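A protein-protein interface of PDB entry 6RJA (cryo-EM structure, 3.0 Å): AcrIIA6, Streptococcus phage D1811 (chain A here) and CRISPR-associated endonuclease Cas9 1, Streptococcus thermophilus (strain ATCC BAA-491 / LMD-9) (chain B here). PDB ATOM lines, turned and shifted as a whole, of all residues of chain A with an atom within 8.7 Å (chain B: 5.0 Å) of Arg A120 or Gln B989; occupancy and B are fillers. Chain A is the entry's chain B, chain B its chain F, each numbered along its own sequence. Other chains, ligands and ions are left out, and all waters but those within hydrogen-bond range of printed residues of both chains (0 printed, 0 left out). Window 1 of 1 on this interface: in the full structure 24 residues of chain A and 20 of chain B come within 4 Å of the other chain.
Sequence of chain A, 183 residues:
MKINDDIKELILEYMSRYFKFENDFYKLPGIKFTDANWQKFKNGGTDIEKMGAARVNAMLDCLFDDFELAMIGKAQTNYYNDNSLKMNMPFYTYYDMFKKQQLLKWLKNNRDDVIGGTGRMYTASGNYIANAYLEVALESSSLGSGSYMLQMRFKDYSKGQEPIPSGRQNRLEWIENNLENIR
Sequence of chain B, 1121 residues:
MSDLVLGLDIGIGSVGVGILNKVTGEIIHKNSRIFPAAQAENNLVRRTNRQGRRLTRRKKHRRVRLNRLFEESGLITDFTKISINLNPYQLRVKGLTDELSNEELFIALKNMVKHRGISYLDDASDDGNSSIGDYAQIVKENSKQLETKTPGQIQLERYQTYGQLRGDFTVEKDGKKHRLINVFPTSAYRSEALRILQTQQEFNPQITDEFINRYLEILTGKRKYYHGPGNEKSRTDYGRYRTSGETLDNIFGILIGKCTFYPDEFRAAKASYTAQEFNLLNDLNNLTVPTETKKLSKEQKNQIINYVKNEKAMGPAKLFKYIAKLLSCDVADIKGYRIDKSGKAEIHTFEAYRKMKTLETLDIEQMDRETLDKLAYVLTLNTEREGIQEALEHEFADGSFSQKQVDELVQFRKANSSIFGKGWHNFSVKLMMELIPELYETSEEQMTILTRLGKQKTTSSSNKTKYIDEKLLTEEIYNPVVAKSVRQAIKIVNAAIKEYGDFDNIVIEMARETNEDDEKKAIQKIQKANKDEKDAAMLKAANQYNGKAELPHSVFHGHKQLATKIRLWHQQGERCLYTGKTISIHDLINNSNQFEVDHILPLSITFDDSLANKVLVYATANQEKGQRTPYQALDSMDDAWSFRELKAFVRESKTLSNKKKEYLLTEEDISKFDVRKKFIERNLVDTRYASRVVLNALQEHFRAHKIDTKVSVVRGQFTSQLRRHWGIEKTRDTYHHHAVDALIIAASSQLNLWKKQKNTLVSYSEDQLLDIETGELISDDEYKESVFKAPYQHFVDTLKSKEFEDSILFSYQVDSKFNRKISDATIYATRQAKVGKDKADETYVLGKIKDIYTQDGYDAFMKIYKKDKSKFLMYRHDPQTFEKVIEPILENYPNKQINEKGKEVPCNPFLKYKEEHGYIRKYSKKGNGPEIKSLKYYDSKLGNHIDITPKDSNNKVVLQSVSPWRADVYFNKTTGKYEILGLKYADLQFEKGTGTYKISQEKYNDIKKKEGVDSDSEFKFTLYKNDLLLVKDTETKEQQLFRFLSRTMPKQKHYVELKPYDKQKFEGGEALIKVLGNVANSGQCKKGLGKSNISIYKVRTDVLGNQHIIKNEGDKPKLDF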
ATOM      1  N   PHE A  19     -13.297  19.378  30.876  1.00  0.00           N
ATOM      2  CA  PHE A  19     -12.419  20.386  30.303  1.00  0.00           C
ATOM      3  C   PHE A  19     -10.989  19.877  30.330  1.00  0.00           C
ATOM      4  O   PHE A  19     -10.584  19.193  31.271  1.00  0.00           O
ATOM      5  CB  PHE A  19     -12.513  21.707  31.068  1.00  0.00           C
ATOM      6  CG  PHE A  19     -13.833  22.400  30.927  1.00  0.00           C
ATOM      7  CD1 PHE A  19     -14.050  23.300  29.902  1.00  0.00           C
ATOM      8  CD2 PHE A  19     -14.856  22.153  31.820  1.00  0.00           C
ATOM      9  CE1 PHE A  19     -15.260  23.935  29.773  1.00  0.00           C
ATOM     10  CE2 PHE A  19     -16.064  22.785  31.693  1.00  0.00           C
ATOM     11  CZ  PHE A  19     -16.263  23.677  30.668  1.00  0.00           C
ATOM     12  N   CYS A  62     -22.951  24.572  35.737  1.00  0.00           N
ATOM     13  CA  CYS A  62     -22.194  24.284  34.524  1.00  0.00           C
ATOM     14  C   CYS A  62     -21.843  22.811  34.424  1.00  0.00           C
ATOM     15  O   CYS A  62     -21.964  22.218  33.348  1.00  0.00           O
ATOM     16  CB  CYS A  62     -20.925  25.127  34.451  1.00  0.00           C
ATOM     17  SG  CYS A  62     -20.043  24.927  32.881  1.00  0.00           S
ATOM     18  N   GLY A 116     -30.399   9.393  22.861  1.00  0.00           N
ATOM     19  CA  GLY A 116     -29.093   9.907  23.211  1.00  0.00           C
ATOM     20  C   GLY A 116     -28.584  10.845  22.144  1.00  0.00           C
ATOM     21  O   GLY A 116     -29.183  10.997  21.081  1.00  0.00           O
ATOM     22  N   GLY A 117     -27.455  11.471  22.443  1.00  0.00           N
ATOM     23  CA  GLY A 117     -26.897  12.446  21.525  1.00  0.00           C
ATOM     24  C   GLY A 117     -25.540  12.920  21.986  1.00  0.00           C
ATOM     25  O   GLY A 117     -25.029  12.504  23.027  1.00  0.00           O
ATOM     26  N   THR A 118     -24.978  13.833  21.205  1.00  0.00           N
ATOM     27  CA  THR A 118     -23.645  14.380  21.427  1.00  0.00           C
ATOM     28  C   THR A 118     -23.753  15.753  22.073  1.00  0.00           C
ATOM     29  O   THR A 118     -24.443  16.633  21.552  1.00  0.00           O
ATOM     30  CB  THR A 118     -22.890  14.459  20.099  1.00  0.00           C
ATOM     31  OG1 THR A 118     -22.424  13.155  19.738  1.00  0.00           O
ATOM     32  CG2 THR A 118     -21.721  15.386  20.173  1.00  0.00           C
ATOM     33  N   GLY A 119     -23.085  15.934  23.207  1.00  0.00           N
ATOM     34  CA  GLY A 119     -23.175  17.160  23.969  1.00  0.00           C
ATOM     35  C   GLY A 119     -22.064  18.145  23.668  1.00  0.00           C
ATOM     36  O   GLY A 119     -20.937  17.768  23.378  1.00  0.00           O
ATOM     37  N   ARG A 120     -22.401  19.422  23.781  1.00  0.00           N
ATOM     38  CA  ARG A 120     -21.594  20.524  23.288  1.00  0.00           C
ATOM     39  C   ARG A 120     -21.476  21.554  24.400  1.00  0.00           C
ATOM     40  O   ARG A 120     -22.484  21.918  25.008  1.00  0.00           O
ATOM     41  CB  ARG A 120     -22.263  21.082  22.034  1.00  0.00           C
ATOM     42  CG  ARG A 120     -21.919  22.461  21.610  1.00  0.00           C
ATOM     43  CD  ARG A 120     -22.887  22.875  20.517  1.00  0.00           C
ATOM     44  NE  ARG A 120     -22.717  22.091  19.301  1.00  0.00           N
ATOM     45  CZ  ARG A 120     -23.172  22.458  18.109  1.00  0.00           C
ATOM     46  NH1 ARG A 120     -22.975  21.689  17.052  1.00  0.00           N
ATOM     47  NH2 ARG A 120     -23.824  23.598  17.973  1.00  0.00           N
ATOM     48  N   MET A 121     -20.260  22.012  24.687  1.00  0.00           N
ATOM     49  CA  MET A 121     -19.992  22.789  25.893  1.00  0.00           C
ATOM     50  C   MET A 121     -19.235  24.064  25.564  1.00  0.00           C
ATOM     51  O   MET A 121     -18.175  24.011  24.941  1.00  0.00           O
ATOM     52  CB  MET A 121     -19.187  21.969  26.898  1.00  0.00           C
ATOM     53  CG  MET A 121     -18.961  22.661  28.217  1.00  0.00           C
ATOM     54  SD  MET A 121     -20.316  22.405  29.371  1.00  0.00           S
ATOM     55  CE  MET A 121     -19.723  20.970  30.248  1.00  0.00           C
ATOM     56  N   TYR A 122     -19.763  25.199  26.011  1.00  0.00           N
ATOM     57  CA  TYR A 122     -19.166  26.499  25.731  1.00  0.00           C
ATOM     58  C   TYR A 122     -18.038  26.824  26.701  1.00  0.00           C
ATOM     59  O   TYR A 122     -18.153  26.606  27.908  1.00  0.00           O
ATOM     60  CB  TYR A 122     -20.233  27.587  25.775  1.00  0.00           C
ATOM     61  CG  TYR A 122     -21.070  27.621  24.524  1.00  0.00           C
ATOM     62  CD1 TYR A 122     -22.108  26.727  24.337  1.00  0.00           C
ATOM     63  CD2 TYR A 122     -20.803  28.530  23.517  1.00  0.00           C
ATOM     64  CE1 TYR A 122     -22.860  26.744  23.192  1.00  0.00           C
ATOM     65  CE2 TYR A 122     -21.552  28.554  22.366  1.00  0.00           C
ATOM     66  CZ  TYR A 122     -22.580  27.661  22.210  1.00  0.00           C
ATOM     67  OH  TYR A 122     -23.334  27.680  21.065  1.00  0.00           O
ATOM     68  N   THR A 123     -16.944  27.355  26.159  1.00  0.00           N
ATOM     69  CA  THR A 123     -15.745  27.701  26.910  1.00  0.00           C
ATOM     70  C   THR A 123     -15.937  29.132  27.444  1.00  0.00           C
ATOM     71  O   THR A 123     -17.041  29.678  27.375  1.00  0.00           O
ATOM     72  CB  THR A 123     -14.553  27.440  25.961  1.00  0.00           C
ATOM     73  OG1 THR A 123     -14.665  26.103  25.470  1.00  0.00           O
ATOM     74  CG2 THR A 123     -13.184  27.509  26.563  1.00  0.00           C
ATOM     75  N   GLY A 126     -16.294  31.904  24.253  1.00  0.00           N
ATOM     76  CA  GLY A 126     -17.415  31.835  23.350  1.00  0.00           C
ATOM     77  C   GLY A 126     -17.388  30.665  22.392  1.00  0.00           C
ATOM     78  O   GLY A 126     -18.424  30.338  21.806  1.00  0.00           O
ATOM     79  N   ASN A 127     -16.242  30.030  22.220  1.00  0.00           N
ATOM     80  CA  ASN A 127     -16.101  28.923  21.296  1.00  0.00           C
ATOM     81  C   ASN A 127     -16.437  27.635  22.022  1.00  0.00           C
ATOM     82  O   ASN A 127     -16.049  27.454  23.168  1.00  0.00           O
ATOM     83  CB  ASN A 127     -14.672  28.881  20.771  1.00  0.00           C
ATOM     84  CG  ASN A 127     -14.104  30.263  20.562  1.00  0.00           C
ATOM     85  OD1 ASN A 127     -14.654  31.065  19.813  1.00  0.00           O
ATOM     86  ND2 ASN A 127     -13.021  30.567  21.254  1.00  0.00           N
ATOM     87  N   TYR A 128     -17.170  26.744  21.373  1.00  0.00           N
ATOM     88  CA  TYR A 128     -17.571  25.561  22.114  1.00  0.00           C
ATOM     89  C   TYR A 128     -16.609  24.404  21.889  1.00  0.00           C
ATOM     90  O   TYR A 128     -15.779  24.416  20.981  1.00  0.00           O
ATOM     91  CB  TYR A 128     -19.004  25.144  21.771  1.00  0.00           C
ATOM     92  CG  TYR A 128     -19.314  24.889  20.320  1.00  0.00           C
ATOM     93  CD1 TYR A 128     -19.075  23.655  19.740  1.00  0.00           C
ATOM     94  CD2 TYR A 128     -19.890  25.872  19.543  1.00  0.00           C
ATOM     95  CE1 TYR A 128     -19.372  23.420  18.421  1.00  0.00           C
ATOM     96  CE2 TYR A 128     -20.195  25.643  18.223  1.00  0.00           C
ATOM     97  CZ  TYR A 128     -19.934  24.416  17.668  1.00  0.00           C
ATOM     98  OH  TYR A 128     -20.238  24.188  16.350  1.00  0.00           O
ATOM     99  N   ILE A 129     -16.712  23.412  22.765  1.00  0.00           N
ATOM    100  CA  ILE A 129     -16.114  22.102  22.547  1.00  0.00           C
ATOM    101  C   ILE A 129     -17.186  21.230  21.916  1.00  0.00           C
ATOM    102  O   ILE A 129     -18.193  20.920  22.552  1.00  0.00           O
ATOM    103  CB  ILE A 129     -15.611  21.482  23.853  1.00  0.00           C
ATOM    104  CG1 ILE A 129     -14.730  22.463  24.612  1.00  0.00           C
ATOM    105  CG2 ILE A 129     -14.861  20.216  23.576  1.00  0.00           C
ATOM    106  CD1 ILE A 129     -14.522  22.083  26.045  1.00  0.00           C
ATOM    107  N   ALA A 130     -16.981  20.831  20.671  1.00  0.00           N
ATOM    108  CA  ALA A 130     -17.863  19.855  20.064  1.00  0.00           C
ATOM    109  C   ALA A 130     -17.521  18.479  20.605  1.00  0.00           C
ATOM    110  O   ALA A 130     -16.343  18.134  20.733  1.00  0.00           O
ATOM    111  CB  ALA A 130     -17.727  19.879  18.546  1.00  0.00           C
ATOM    112  N   ASN A 131     -18.561  17.710  20.942  1.00  0.00           N
ATOM    113  CA  ASN A 131     -18.466  16.380  21.550  1.00  0.00           C
ATOM    114  C   ASN A 131     -17.696  16.422  22.873  1.00  0.00           C
ATOM    115  O   ASN A 131     -16.593  15.897  23.011  1.00  0.00           O
ATOM    116  CB  ASN A 131     -17.864  15.361  20.575  1.00  0.00           C
ATOM    117  CG  ASN A 131     -18.047  13.941  21.035  1.00  0.00           C
ATOM    118  OD1 ASN A 131     -18.850  13.660  21.918  1.00  0.00           O
ATOM    119  ND2 ASN A 131     -17.302  13.034  20.434  1.00  0.00           N
ATOM    120  N   ALA A 132     -18.319  17.075  23.850  1.00  0.00           N
ATOM    121  CA  ALA A 132     -17.796  17.074  25.209  1.00  0.00           C
ATOM    122  C   ALA A 132     -18.275  15.878  26.020  1.00  0.00           C
ATOM    123  O   ALA A 132     -17.518  15.350  26.839  1.00  0.00           O
ATOM    124  CB  ALA A 132     -18.180  18.369  25.925  1.00  0.00           C
ATOM    125  N   TYR A 133     -19.514  15.433  25.813  1.00  0.00           N
ATOM    126  CA  TYR A 133     -20.078  14.336  26.588  1.00  0.00           C
ATOM    127  C   TYR A 133     -21.147  13.625  25.768  1.00  0.00           C
ATOM    128  O   TYR A 133     -21.427  13.985  24.623  1.00  0.00           O
ATOM    129  CB  TYR A 133     -20.647  14.836  27.921  1.00  0.00           C
ATOM    130  CG  TYR A 133     -21.528  16.060  27.832  1.00  0.00           C
ATOM    131  CD1 TYR A 133     -22.875  15.948  27.559  1.00  0.00           C
ATOM    132  CD2 TYR A 133     -21.014  17.324  28.052  1.00  0.00           C
ATOM    133  CE1 TYR A 133     -23.676  17.048  27.490  1.00  0.00           C
ATOM    134  CE2 TYR A 133     -21.814  18.433  27.979  1.00  0.00           C
ATOM    135  CZ  TYR A 133     -23.146  18.287  27.694  1.00  0.00           C
ATOM    136  OH  TYR A 133     -23.964  19.387  27.620  1.00  0.00           O
ATOM    137  N   LEU A 134     -21.779  12.634  26.391  1.00  0.00           N
ATOM    138  CA  LEU A 134     -22.871  11.865  25.807  1.00  0.00           C
ATOM    139  C   LEU A 134     -24.141  12.124  26.605  1.00  0.00           C
ATOM    140  O   LEU A 134     -24.183  11.846  27.807  1.00  0.00           O
ATOM    141  CB  LEU A 134     -22.533  10.375  25.813  1.00  0.00           C
ATOM    142  CG  LEU A 134     -23.594   9.351  25.423  1.00  0.00           C
ATOM    143  CD1 LEU A 134     -23.982   9.460  23.967  1.00  0.00           C
ATOM    144  CD2 LEU A 134     -23.107   7.956  25.749  1.00  0.00           C
ATOM    145  N   GLU A 135     -25.171  12.648  25.945  1.00  0.00           N
ATOM    146  CA  GLU A 135     -26.456  12.906  26.583  1.00  0.00           C
ATOM    147  C   GLU A 135     -27.356  11.692  26.446  1.00  0.00           C
ATOM    148  O   GLU A 135     -27.466  11.131  25.355  1.00  0.00           O
ATOM    149  CB  GLU A 135     -27.147  14.102  25.941  1.00  0.00           C
ATOM    150  CG  GLU A 135     -26.601  15.439  26.323  1.00  0.00           C
ATOM    151  CD  GLU A 135     -27.190  16.560  25.490  1.00  0.00           C
ATOM    152  OE1 GLU A 135     -27.557  16.303  24.323  1.00  0.00           O
ATOM    153  OE2 GLU A 135     -27.284  17.699  25.997  1.00  0.00           O
ATOM    154  N   ARG A 153     -25.891  12.363  31.750  1.00  0.00           N
ATOM    155  CA  ARG A 153     -24.731  12.919  31.068  1.00  0.00           C
ATOM    156  C   ARG A 153     -23.513  12.072  31.401  1.00  0.00           C
ATOM    157  O   ARG A 153     -23.117  12.001  32.566  1.00  0.00           O
ATOM    158  CB  ARG A 153     -24.557  14.364  31.524  1.00  0.00           C
ATOM    159  CG  ARG A 153     -23.430  15.136  30.952  1.00  0.00           C
ATOM    160  CD  ARG A 153     -23.309  16.461  31.676  1.00  0.00           C
ATOM    161  NE  ARG A 153     -24.381  17.386  31.334  1.00  0.00           N
ATOM    162  CZ  ARG A 153     -24.241  18.706  31.301  1.00  0.00           C
ATOM    163  NH1 ARG A 153     -23.074  19.254  31.577  1.00  0.00           N
ATOM    164  NH2 ARG A 153     -25.264  19.480  30.985  1.00  0.00           N
ATOM    165  N   ALA B 986     -22.708  27.961  13.141  1.00  0.00           N
ATOM    166  CA  ALA B 986     -22.358  26.739  13.840  1.00  0.00           C
ATOM    167  C   ALA B 986     -22.935  26.672  15.242  1.00  0.00           C
ATOM    168  O   ALA B 986     -22.565  25.777  16.003  1.00  0.00           O
ATOM    169  CB  ALA B 986     -20.840  26.590  13.900  1.00  0.00           C
ATOM    170  N   ASP B 987     -23.821  27.592  15.604  1.00  0.00           N
ATOM    171  CA  ASP B 987     -24.505  27.530  16.886  1.00  0.00           C
ATOM    172  C   ASP B 987     -25.783  26.710  16.834  1.00  0.00           C
ATOM    173  O   ASP B 987     -26.395  26.479  17.879  1.00  0.00           O
ATOM    174  CB  ASP B 987     -24.825  28.939  17.384  1.00  0.00           C
ATOM    175  CG  ASP B 987     -23.598  29.674  17.862  1.00  0.00           C
ATOM    176  OD1 ASP B 987     -22.540  29.032  17.992  1.00  0.00           O
ATOM    177  OD2 ASP B 987     -23.682  30.891  18.114  1.00  0.00           O
ATOM    178  N   LEU B 988     -26.190  26.261  15.656  1.00  0.00           N
ATOM    179  CA  LEU B 988     -27.375  25.439  15.492  1.00  0.00           C
ATOM    180  C   LEU B 988     -26.956  23.990  15.296  1.00  0.00           C
ATOM    181  O   LEU B 988     -25.780  23.682  15.123  1.00  0.00           O
ATOM    182  CB  LEU B 988     -28.213  25.936  14.316  1.00  0.00           C
ATOM    183  CG  LEU B 988     -29.182  27.082  14.612  1.00  0.00           C
ATOM    184  CD1 LEU B 988     -28.488  28.417  14.640  1.00  0.00           C
ATOM    185  CD2 LEU B 988     -30.294  27.102  13.597  1.00  0.00           C
ATOM    186  N   GLN B 989     -27.934  23.091  15.312  1.00  0.00           N
ATOM    187  CA  GLN B 989     -27.598  21.678  15.368  1.00  0.00           C
ATOM    188  C   GLN B 989     -28.780  20.861  14.868  1.00  0.00           C
ATOM    189  O   GLN B 989     -29.933  21.259  15.034  1.00  0.00           O
ATOM    190  CB  GLN B 989     -27.243  21.293  16.810  1.00  0.00           C
ATOM    191  CG  GLN B 989     -26.659  19.921  17.022  1.00  0.00           C
ATOM    192  CD  GLN B 989     -26.237  19.712  18.448  1.00  0.00           C
ATOM    193  OE1 GLN B 989     -26.343  20.618  19.269  1.00  0.00           O
ATOM    194  NE2 GLN B 989     -25.713  18.535  18.747  1.00  0.00           N
ATOM    195  N   PHE B 990     -28.487  19.717  14.254  1.00  0.00           N
ATOM    196  CA  PHE B 990     -29.489  18.672  14.099  1.00  0.00           C
ATOM    197  C   PHE B 990     -29.660  17.968  15.438  1.00  0.00           C
ATOM    198  O   PHE B 990     -28.683  17.505  16.028  1.00  0.00           O
ATOM    199  CB  PHE B 990     -29.080  17.669  13.023  1.00  0.00           C
ATOM    200  CG  PHE B 990     -29.136  18.211  11.630  1.00  0.00           C
ATOM    201  CD1 PHE B 990     -30.344  18.366  10.983  1.00  0.00           C
ATOM    202  CD2 PHE B 990     -27.976  18.558  10.963  1.00  0.00           C
ATOM    203  CE1 PHE B 990     -30.396  18.871   9.701  1.00  0.00           C
ATOM    204  CE2 PHE B 990     -28.027  19.061   9.680  1.00  0.00           C
ATOM    205  CZ  PHE B 990     -29.236  19.217   9.054  1.00  0.00           C
ATOM    206  N   GLU B 991     -30.893  17.887  15.919  1.00  0.00           N
ATOM    207  CA  GLU B 991     -31.121  17.441  17.283  1.00  0.00           C
ATOM    208  C   GLU B 991     -31.313  15.932  17.359  1.00  0.00           C
ATOM    209  O   GLU B 991     -31.434  15.238  16.353  1.00  0.00           O
ATOM    210  CB  GLU B 991     -32.312  18.168  17.879  1.00  0.00           C
ATOM    211  CG  GLU B 991     -32.080  19.644  17.939  1.00  0.00           C
ATOM    212  CD  GLU B 991     -31.429  20.087  19.225  1.00  0.00           C
ATOM    213  OE1 GLU B 991     -32.025  19.866  20.297  1.00  0.00           O
ATOM    214  OE2 GLU B 991     -30.323  20.657  19.168  1.00  0.00           O
ATOM    215  N   THR B 996     -34.402  17.649  13.851  1.00  0.00           N
ATOM    216  CA  THR B 996     -34.758  19.006  13.481  1.00  0.00           C
ATOM    217  C   THR B 996     -33.556  19.920  13.650  1.00  0.00           C
ATOM    218  O   THR B 996     -32.639  19.639  14.421  1.00  0.00           O
ATOM    219  CB  THR B 996     -35.921  19.512  14.327  1.00  0.00           C
ATOM    220  OG1 THR B 996     -35.739  19.091  15.681  1.00  0.00           O
ATOM    221  CG2 THR B 996     -37.234  18.965  13.805  1.00  0.00           C
ATOM    222  N   TYR B 997     -33.575  21.030  12.925  1.00  0.00           N
ATOM    223  CA  TYR B 997     -32.482  21.992  12.934  1.00  0.00           C
ATOM    224  C   TYR B 997     -32.881  23.154  13.832  1.00  0.00           C
ATOM    225  O   TYR B 997     -33.726  23.968  13.457  1.00  0.00           O
ATOM    226  CB  TYR B 997     -32.178  22.469  11.516  1.00  0.00           C
ATOM    227  CG  TYR B 997     -30.783  23.007  11.328  1.00  0.00           C
ATOM    228  CD1 TYR B 997     -29.685  22.167  11.366  1.00  0.00           C
ATOM    229  CD2 TYR B 997     -30.563  24.352  11.109  1.00  0.00           C
ATOM    230  CE1 TYR B 997     -28.414  22.653  11.198  1.00  0.00           C
ATOM    231  CE2 TYR B 997     -29.293  24.842  10.942  1.00  0.00           C
ATOM    232  CZ  TYR B 997     -28.225  23.988  10.988  1.00  0.00           C
ATOM    233  OH  TYR B 997     -26.956  24.478  10.816  1.00  0.00           O
ATOM    234  N   LYS B 998     -32.264  23.237  15.007  1.00  0.00           N
ATOM    235  CA  LYS B 998     -32.617  24.255  15.984  1.00  0.00           C
ATOM    236  C   LYS B 998     -31.508  24.362  17.018  1.00  0.00           C
ATOM    237  O   LYS B 998     -30.571  23.564  17.039  1.00  0.00           O
ATOM    238  CB  LYS B 998     -33.942  23.929  16.669  1.00  0.00           C
ATOM    239  CG  LYS B 998     -33.867  22.769  17.609  1.00  0.00           C
ATOM    240  CD  LYS B 998     -35.236  22.281  17.993  1.00  0.00           C
ATOM    241  CE  LYS B 998     -35.153  21.318  19.147  1.00  0.00           C
ATOM    242  NZ  LYS B 998     -34.087  21.716  20.096  1.00  0.00           N
ATOM    243  N   LYS B1003     -28.276  26.261  25.738  1.00  0.00           N
ATOM    244  CA  LYS B1003     -27.149  26.798  24.988  1.00  0.00           C
ATOM    245  C   LYS B1003     -27.376  28.257  24.628  1.00  0.00           C
ATOM    246  O   LYS B1003     -26.429  29.052  24.617  1.00  0.00           O
ATOM    247  CB  LYS B1003     -26.917  25.973  23.728  1.00  0.00           C
ATOM    248  CG  LYS B1003     -26.762  24.490  23.970  1.00  0.00           C
ATOM    249  CD  LYS B1003     -25.614  24.197  24.904  1.00  0.00           C
ATOM    250  CE  LYS B1003     -25.639  22.751  25.347  1.00  0.00           C
ATOM    251  NZ  LYS B1003     -24.847  22.533  26.584  1.00  0.00           N
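OH of Tyr A133 lies within hydrogen-bond range of NZ of Lys B1003, at 3.4 Å.
The guanidinium group of Arg A120 is in hydrogen-bond range of the backbone carbonyl oxygen of Ala B986 (3.2 Å).
O of Arg A120 lies within hydrogen-bond range of NZ of Lys B1003 (2.9 Å).
The side-chain hydroxyl (OH) of Tyr A128 lies within hydrogen-bond range of the backbone carbonyl oxygen (O) of Ala B986, 2.8 Å away.
NH2 of Arg A120 is in hydrogen-bond range of O of Leu B988, at 3.5 Å.
OH of Tyr A122 sits at hydrogen-bond distance from OD1 of Asp B987 (3.4 Å).
N of Gly A119 is in hydrogen-bond range of O of Tyr A133 (2.9 Å).
The backbone NH (N) of Lys B998 is in hydrogen-bond range of the backbone carbonyl oxygen (O) of Gln B989 (3.1 Å).
Hydrophobic or aromatic side chains of chain B that line the printed part of chain A: Ala B986.
Hydrophobic or aromatic side chains of chain A that line the printed part of chain B: Tyr A122, Tyr A128 and Tyr A133.
Among the printed residues, 9 pairs touch across the chains.
Among the printed residues, no Asp or Glu carboxylate lies within 4 Å of a Lys or Arg side-chain nitrogen of the other chain.
Among the printed residues, merely in contact across the chains: Thr A118 with Gln B989 (3.6 Å), Arg A120 with Asp B987 (3.8 Å) and Arg A120 with Gln B989 (3.8 Å).
Of the printed residues of chain B, Tyr A128 touches Ala B986.
Printed residues of chain A within 4 Å of Ala B986: Arg A120 and Tyr A128.
Of the printed residues of chain A, Leu B988 touches Arg A120.
Printed residues of chain B within 4 Å of Tyr A133: Lys B1003 (3.4 Å).
Printed residues of chain B within 4 Å of Tyr A122: Asp B987 (3.4 Å).
Asn A127 touches none of the printed residues of chain B.
The nearest printed residue of chain B that does not touch Tyr A128 is Asp B987 (4.1 Å).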
